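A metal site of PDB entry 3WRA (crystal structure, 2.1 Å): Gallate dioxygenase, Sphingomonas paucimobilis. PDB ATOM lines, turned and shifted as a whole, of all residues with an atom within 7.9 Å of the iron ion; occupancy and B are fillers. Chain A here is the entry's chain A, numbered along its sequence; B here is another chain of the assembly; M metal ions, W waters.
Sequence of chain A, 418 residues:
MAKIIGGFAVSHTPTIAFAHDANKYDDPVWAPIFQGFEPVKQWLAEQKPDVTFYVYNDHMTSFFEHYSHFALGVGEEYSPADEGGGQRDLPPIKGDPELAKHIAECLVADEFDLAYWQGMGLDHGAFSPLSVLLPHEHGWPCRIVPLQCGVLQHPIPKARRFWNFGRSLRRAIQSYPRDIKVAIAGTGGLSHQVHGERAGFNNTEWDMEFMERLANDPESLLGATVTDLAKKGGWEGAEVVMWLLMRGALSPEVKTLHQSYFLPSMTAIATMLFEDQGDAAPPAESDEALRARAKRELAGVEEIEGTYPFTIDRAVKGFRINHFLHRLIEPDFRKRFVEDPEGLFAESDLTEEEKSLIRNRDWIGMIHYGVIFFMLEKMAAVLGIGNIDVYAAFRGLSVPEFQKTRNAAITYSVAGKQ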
ATOM      1  N   SER A  11       7.218  16.298  10.393  1.00  0.00           N
ATOM      2  CA  SER A  11       6.812  14.984   9.876  1.00  0.00           C
ATOM      3  C   SER A  11       8.031  14.082   9.855  1.00  0.00           C
ATOM      4  O   SER A  11       9.152  14.572   9.861  1.00  0.00           O
ATOM      5  CB  SER A  11       6.235  15.137   8.474  1.00  0.00           C
ATOM      6  OG  SER A  11       5.026  15.889   8.528  1.00  0.00           O
ATOM      7  N   HIS A  12       7.846  12.758   9.874  1.00  0.00           N
ATOM      8  CA  HIS A  12       9.049  11.903   9.846  1.00  0.00           C
ATOM      9  C   HIS A  12       9.100  10.797   8.792  1.00  0.00           C
ATOM     10  O   HIS A  12       9.924   9.892   8.919  1.00  0.00           O
ATOM     11  CB  HIS A  12       9.492  11.410  11.248  1.00  0.00           C
ATOM     12  CG  HIS A  12       8.504  10.526  11.962  1.00  0.00           C
ATOM     13  ND1 HIS A  12       8.449  10.435  13.331  1.00  0.00           N
ATOM     14  CD2 HIS A  12       7.548   9.687  11.489  1.00  0.00           C
ATOM     15  CE1 HIS A  12       7.490   9.594  13.677  1.00  0.00           C
ATOM     16  NE2 HIS A  12       6.931   9.119  12.576  1.00  0.00           N
ATOM     17  N   THR A  13       8.268  10.922   7.739  1.00  0.00           N
ATOM     18  CA  THR A  13       8.271  10.009   6.580  1.00  0.00           C
ATOM     19  C   THR A  13       9.671   9.634   6.103  1.00  0.00           C
ATOM     20  O   THR A  13      10.556  10.505   6.074  1.00  0.00           O
ATOM     21  CB  THR A  13       7.584  10.628   5.305  1.00  0.00           C
ATOM     22  OG1 THR A  13       6.888  11.850   5.617  1.00  0.00           O
ATOM     23  CG2 THR A  13       6.676   9.595   4.606  1.00  0.00           C
ATOM     24  N   PRO A  14       9.864   8.353   5.699  1.00  0.00           N
ATOM     25  CA  PRO A  14      11.067   7.907   4.989  1.00  0.00           C
ATOM     26  C   PRO A  14      11.429   8.751   3.742  1.00  0.00           C
ATOM     27  O   PRO A  14      12.611   8.785   3.349  1.00  0.00           O
ATOM     28  CB  PRO A  14      10.706   6.475   4.545  1.00  0.00           C
ATOM     29  CG  PRO A  14       9.708   6.013   5.546  1.00  0.00           C
ATOM     30  CD  PRO A  14       8.924   7.245   5.959  1.00  0.00           C
ATOM     31  N   TYR A  56       9.250  10.315  18.941  1.00  0.00           N
ATOM     32  CA  TYR A  56       8.971   9.667  17.669  1.00  0.00           C
ATOM     33  C   TYR A  56       8.308   8.320  17.914  1.00  0.00           C
ATOM     34  O   TYR A  56       8.171   7.892  19.062  1.00  0.00           O
ATOM     35  CB  TYR A  56      10.291   9.466  16.903  1.00  0.00           C
ATOM     36  CG  TYR A  56      11.119   8.277  17.390  1.00  0.00           C
ATOM     37  CD1 TYR A  56      11.270   7.153  16.590  1.00  0.00           C
ATOM     38  CD2 TYR A  56      11.736   8.293  18.654  1.00  0.00           C
ATOM     39  CE1 TYR A  56      12.005   6.044  17.028  1.00  0.00           C
ATOM     40  CE2 TYR A  56      12.483   7.175  19.099  1.00  0.00           C
ATOM     41  CZ  TYR A  56      12.609   6.062  18.274  1.00  0.00           C
ATOM     42  OH  TYR A  56      13.327   4.953  18.670  1.00  0.00           O
ATOM     43  N   ASN A  57       7.880   7.663  16.829  1.00  0.00           N
ATOM     44  CA  ASN A  57       7.524   6.249  16.943  1.00  0.00           C
ATOM     45  C   ASN A  57       8.375   5.406  16.017  1.00  0.00           C
ATOM     46  O   ASN A  57       8.780   5.871  14.940  1.00  0.00           O
ATOM     47  CB  ASN A  57       6.015   5.984  16.772  1.00  0.00           C
ATOM     48  CG  ASN A  57       5.555   6.057  15.334  1.00  0.00           C
ATOM     49  OD1 ASN A  57       5.522   7.135  14.723  1.00  0.00           O
ATOM     50  ND2 ASN A  57       5.199   4.912  14.775  1.00  0.00           N
ATOM     51  N   ASP A  58       8.691   4.211  16.472  1.00  0.00           N
ATOM     52  CA  ASP A  58       9.471   3.232  15.744  1.00  0.00           C
ATOM     53  C   ASP A  58       8.463   2.544  14.828  1.00  0.00           C
ATOM     54  O   ASP A  58       7.339   2.312  15.228  1.00  0.00           O
ATOM     55  CB  ASP A  58      10.040   2.227  16.753  1.00  0.00           C
ATOM     56  CG  ASP A  58      10.759   1.083  16.108  1.00  0.00           C
ATOM     57  OD1 ASP A  58      11.942   1.243  15.759  1.00  0.00           O
ATOM     58  OD2 ASP A  58      10.151  -0.002  15.958  1.00  0.00           O
ATOM     59  N   HIS A  59       8.843   2.233  13.595  1.00  0.00           N
ATOM     60  CA  HIS A  59       7.864   1.683  12.674  1.00  0.00           C
ATOM     61  C   HIS A  59       7.958   0.163  12.561  1.00  0.00           C
ATOM     62  O   HIS A  59       8.173  -0.421  11.479  1.00  0.00           O
ATOM     63  CB  HIS A  59       7.896   2.438  11.353  1.00  0.00           C
ATOM     64  CG  HIS A  59       7.522   3.881  11.531  1.00  0.00           C
ATOM     65  ND1 HIS A  59       8.423   4.833  11.960  1.00  0.00           N
ATOM     66  CD2 HIS A  59       6.322   4.501  11.443  1.00  0.00           C
ATOM     67  CE1 HIS A  59       7.790   5.994  12.086  1.00  0.00           C
ATOM     68  NE2 HIS A  59       6.517   5.808  11.786  1.00  0.00           N
ATOM     69  N   ASP A 123      15.088   4.235  14.233  1.00  0.00           N
ATOM     70  CA  ASP A 123      14.701   4.086  12.828  1.00  0.00           C
ATOM     71  C   ASP A 123      14.490   5.463  12.163  1.00  0.00           C
ATOM     72  O   ASP A 123      14.847   6.500  12.743  1.00  0.00           O
ATOM     73  CB  ASP A 123      13.535   3.098  12.642  1.00  0.00           C
ATOM     74  CG  ASP A 123      12.186   3.693  12.990  1.00  0.00           C
ATOM     75  OD1 ASP A 123      12.169   4.721  13.715  1.00  0.00           O
ATOM     76  OD2 ASP A 123      11.131   3.129  12.560  1.00  0.00           O
ATOM     77  N   HIS A 124      13.906   5.486  10.966  1.00  0.00           N
ATOM     78  CA  HIS A 124      13.682   6.724  10.216  1.00  0.00           C
ATOM     79  C   HIS A 124      12.812   7.740  10.957  1.00  0.00           C
ATOM     80  O   HIS A 124      12.702   8.905  10.548  1.00  0.00           O
ATOM     81  CB  HIS A 124      13.067   6.403   8.857  1.00  0.00           C
ATOM     82  CG  HIS A 124      11.641   5.964   8.940  1.00  0.00           C
ATOM     83  ND1 HIS A 124      11.266   4.639   8.926  1.00  0.00           N
ATOM     84  CD2 HIS A 124      10.494   6.676   9.040  1.00  0.00           C
ATOM     85  CE1 HIS A 124       9.955   4.546   8.996  1.00  0.00           C
ATOM     86  NE2 HIS A 124       9.456   5.774   9.074  1.00  0.00           N
ATOM     87  N   GLY A 125      12.181   7.329  12.058  1.00  0.00           N
ATOM     88  CA  GLY A 125      11.363   8.260  12.832  1.00  0.00           C
ATOM     89  C   GLY A 125      12.243   9.362  13.390  1.00  0.00           C
ATOM     90  O   GLY A 125      11.798  10.508  13.560  1.00  0.00           O
ATOM     91  N   CYS A 149       7.278   6.290  21.280  1.00  0.00           N
ATOM     92  CA  CYS A 149       5.901   6.209  21.714  1.00  0.00           C
ATOM     93  C   CYS A 149       5.204   5.137  20.939  1.00  0.00           C
ATOM     94  O   CYS A 149       5.189   5.176  19.712  1.00  0.00           O
ATOM     95  CB  CYS A 149       5.207   7.549  21.454  1.00  0.00           C
ATOM     96  SG  CYS A 149       5.932   8.833  22.429  1.00  0.00           S
ATOM     97  N   VAL A 151       2.448   4.087  19.387  1.00  0.00           N
ATOM     98  CA  VAL A 151       1.214   4.705  18.883  1.00  0.00           C
ATOM     99  C   VAL A 151       0.482   3.791  17.916  1.00  0.00           C
ATOM    100  O   VAL A 151      -0.598   4.146  17.457  1.00  0.00           O
ATOM    101  CB  VAL A 151       1.486   6.073  18.166  1.00  0.00           C
ATOM    102  CG1 VAL A 151       2.008   7.118  19.148  1.00  0.00           C
ATOM    103  CG2 VAL A 151       2.439   5.906  16.988  1.00  0.00           C
ATOM    104  N   LEU A 152       1.084   2.643  17.618  1.00  0.00           N
ATOM    105  CA  LEU A 152       0.589   1.741  16.584  1.00  0.00           C
ATOM    106  C   LEU A 152      -0.334   0.568  17.025  1.00  0.00           C
ATOM    107  O   LEU A 152      -1.175   0.106  16.237  1.00  0.00           O
ATOM    108  CB  LEU A 152       1.756   1.191  15.781  1.00  0.00           C
ATOM    109  CG  LEU A 152       2.720   2.198  15.137  1.00  0.00           C
ATOM    110  CD1 LEU A 152       3.793   1.437  14.412  1.00  0.00           C
ATOM    111  CD2 LEU A 152       1.992   3.156  14.162  1.00  0.00           C
ATOM    112  N   THR A 187       7.575  14.561  16.427  1.00  0.00           N
ATOM    113  CA  THR A 187       7.624  14.127  15.034  1.00  0.00           C
ATOM    114  C   THR A 187       6.465  13.259  14.556  1.00  0.00           C
ATOM    115  O   THR A 187       5.596  12.895  15.318  1.00  0.00           O
ATOM    116  CB  THR A 187       8.958  13.455  14.694  1.00  0.00           C
ATOM    117  OG1 THR A 187       8.941  12.102  15.172  1.00  0.00           O
ATOM    118  CG2 THR A 187      10.108  14.231  15.361  1.00  0.00           C
ATOM    119  N   GLY A 188       6.463  12.929  13.270  1.00  0.00           N
ATOM    120  CA  GLY A 188       5.344  12.238  12.649  1.00  0.00           C
ATOM    121  C   GLY A 188       4.290  13.250  12.238  1.00  0.00           C
ATOM    122  O   GLY A 188       4.459  14.479  12.418  1.00  0.00           O
ATOM    123  N   GLY A 189       3.196  12.734  11.688  1.00  0.00           N
ATOM    124  CA  GLY A 189       2.120  13.555  11.165  1.00  0.00           C
ATOM    125  C   GLY A 189       2.479  14.076   9.775  1.00  0.00           C
ATOM    126  O   GLY A 189       3.584  13.848   9.316  1.00  0.00           O
ATOM    127  N   HIS A 192      -2.590  11.380   7.113  1.00  0.00           N
ATOM    128  CA  HIS A 192      -2.273  10.281   6.192  1.00  0.00           C
ATOM    129  C   HIS A 192      -2.850   8.947   6.644  1.00  0.00           C
ATOM    130  O   HIS A 192      -3.107   8.730   7.842  1.00  0.00           O
ATOM    131  CB  HIS A 192      -0.756  10.159   5.925  1.00  0.00           C
ATOM    132  CG  HIS A 192       0.049   9.683   7.101  1.00  0.00           C
ATOM    133  ND1 HIS A 192       0.265  10.461   8.223  1.00  0.00           N
ATOM    134  CD2 HIS A 192       0.739   8.526   7.306  1.00  0.00           C
ATOM    135  CE1 HIS A 192       1.035   9.791   9.076  1.00  0.00           C
ATOM    136  NE2 HIS A 192       1.331   8.623   8.541  1.00  0.00           N
ATOM    137  N   GLU A 236      -2.920   6.375  10.411  1.00  0.00           N
ATOM    138  CA  GLU A 236      -1.563   6.604  10.907  1.00  0.00           C
ATOM    139  C   GLU A 236      -1.363   8.084  11.237  1.00  0.00           C
ATOM    140  O   GLU A 236      -0.490   8.452  12.038  1.00  0.00           O
ATOM    141  CB  GLU A 236      -0.553   6.056   9.902  1.00  0.00           C
ATOM    142  CG  GLU A 236      -0.556   4.484   9.778  1.00  0.00           C
ATOM    143  CD  GLU A 236      -1.726   3.912   8.956  1.00  0.00           C
ATOM    144  OE1 GLU A 236      -2.585   4.684   8.491  1.00  0.00           O
ATOM    145  OE2 GLU A 236      -1.781   2.664   8.759  1.00  0.00           O
ATOM    146  N   GLY A 237      -2.217   8.933  10.669  1.00  0.00           N
ATOM    147  CA  GLY A 237      -2.225  10.357  10.951  1.00  0.00           C
ATOM    148  C   GLY A 237      -2.501  10.666  12.410  1.00  0.00           C
ATOM    149  O   GLY A 237      -2.116  11.737  12.901  1.00  0.00           O
ATOM    150  N   GLU A 239      -1.044   9.703  14.848  1.00  0.00           N
ATOM    151  CA  GLU A 239       0.222   9.781  15.586  1.00  0.00           C
ATOM    152  C   GLU A 239       0.548  11.212  16.021  1.00  0.00           C
ATOM    153  O   GLU A 239       1.537  11.428  16.733  1.00  0.00           O
ATOM    154  CB  GLU A 239       1.370   9.175  14.769  1.00  0.00           C
ATOM    155  CG  GLU A 239       1.675   9.908  13.483  1.00  0.00           C
ATOM    156  CD  GLU A 239       2.898   9.394  12.786  1.00  0.00           C
ATOM    157  OE1 GLU A 239       3.648   8.639  13.414  1.00  0.00           O
ATOM    158  OE2 GLU A 239       3.118   9.749  11.604  1.00  0.00           O
ATOM    159  N   VAL A 240      -0.275  12.188  15.617  1.00  0.00           N
ATOM    160  CA  VAL A 240      -0.070  13.586  16.026  1.00  0.00           C
ATOM    161  C   VAL A 240      -0.160  13.795  17.526  1.00  0.00           C
ATOM    162  O   VAL A 240       0.240  14.850  18.053  1.00  0.00           O
ATOM    163  CB  VAL A 240      -1.023  14.566  15.300  1.00  0.00           C
ATOM    164  CG1 VAL A 240      -0.724  14.615  13.823  1.00  0.00           C
ATOM    165  CG2 VAL A 240      -2.480  14.179  15.526  1.00  0.00           C
ATOM    166  N   MET A 242       1.742  12.640  19.497  1.00  0.00           N
ATOM    167  CA  MET A 242       3.137  12.912  19.813  1.00  0.00           C
ATOM    168  C   MET A 242       3.489  14.397  19.787  1.00  0.00           C
ATOM    169  O   MET A 242       4.275  14.850  20.622  1.00  0.00           O
ATOM    170  CB  MET A 242       4.047  12.133  18.854  1.00  0.00           C
ATOM    171  CG  MET A 242       4.103  10.639  19.192  1.00  0.00           C
ATOM    172  SD  MET A 242       5.276   9.676  18.206  1.00  0.00           S
ATOM    173  CE  MET A 242       4.539   9.758  16.564  1.00  0.00           C
ATOM    174  N   PHE B 374       3.516  -1.763   8.387  1.00  0.00           N
ATOM    175  CA  PHE B 374       4.991  -1.576   8.466  1.00  0.00           C
ATOM    176  C   PHE B 374       5.799  -2.848   8.200  1.00  0.00           C
ATOM    177  O   PHE B 374       6.987  -2.772   7.855  1.00  0.00           O
ATOM    178  CB  PHE B 374       5.359  -0.880   9.760  1.00  0.00           C
ATOM    179  CG  PHE B 374       4.546   0.357   9.973  1.00  0.00           C
ATOM    180  CD1 PHE B 374       4.782   1.506   9.189  1.00  0.00           C
ATOM    181  CD2 PHE B 374       3.464   0.358  10.865  1.00  0.00           C
ATOM    182  CE1 PHE B 374       4.002   2.640   9.328  1.00  0.00           C
ATOM    183  CE2 PHE B 374       2.670   1.502  11.014  1.00  0.00           C
ATOM    184  CZ  PHE B 374       2.948   2.646  10.235  1.00  0.00           C
HETATM  185 FE    FE M   1       5.245   7.452  12.602  1.00  0.00          FE
HETATM  186  O   HOH W   1       4.734   8.036  10.515  1.00  0.00           O
HETATM  187  O   HOH W   2       3.435   6.056  12.366  1.00  0.00           O
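ND1 of His 12 is in hydrogen-bond range of OG1 of Thr 187 (2.5 Å).
The side-chain sulfur of Met 242 is in hydrogen-bond range of the backbone NH of Asn 57, at 3.6 Å.
ND1 of His 12 is in hydrogen-bond range of N of Gly 188, 3.2 Å away.
OE2 of Glu 239 lies within hydrogen-bond range of N of Gly 189 (3.0 Å).
The side-chain carboxylate (OD2) of Asp 123 is in hydrogen-bond range of the backbone NH (N) of His 59 (2.7 Å).
A ring nitrogen (ND1) of His 12 is in hydrogen-bond range of the backbone carbonyl oxygen (O) of Gly 125, at 3.4 Å.
A ring nitrogen (ND1) of His 59 is in hydrogen-bond range of a ring nitrogen (NE2) of His 124, 3.2 Å away.
Four residues have an atom within 4 Å of the iron ion: His 12, Asn 57, His 59 and Glu 239.
The nearest printed residue that does not touch the iron ion is Met 242 (4.6 Å).
The iron ion is bound by OE1 of Glu 239, OD1 of Asn 57, water W1, NE2 of His 59, water W2 and NE2 of His 12.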
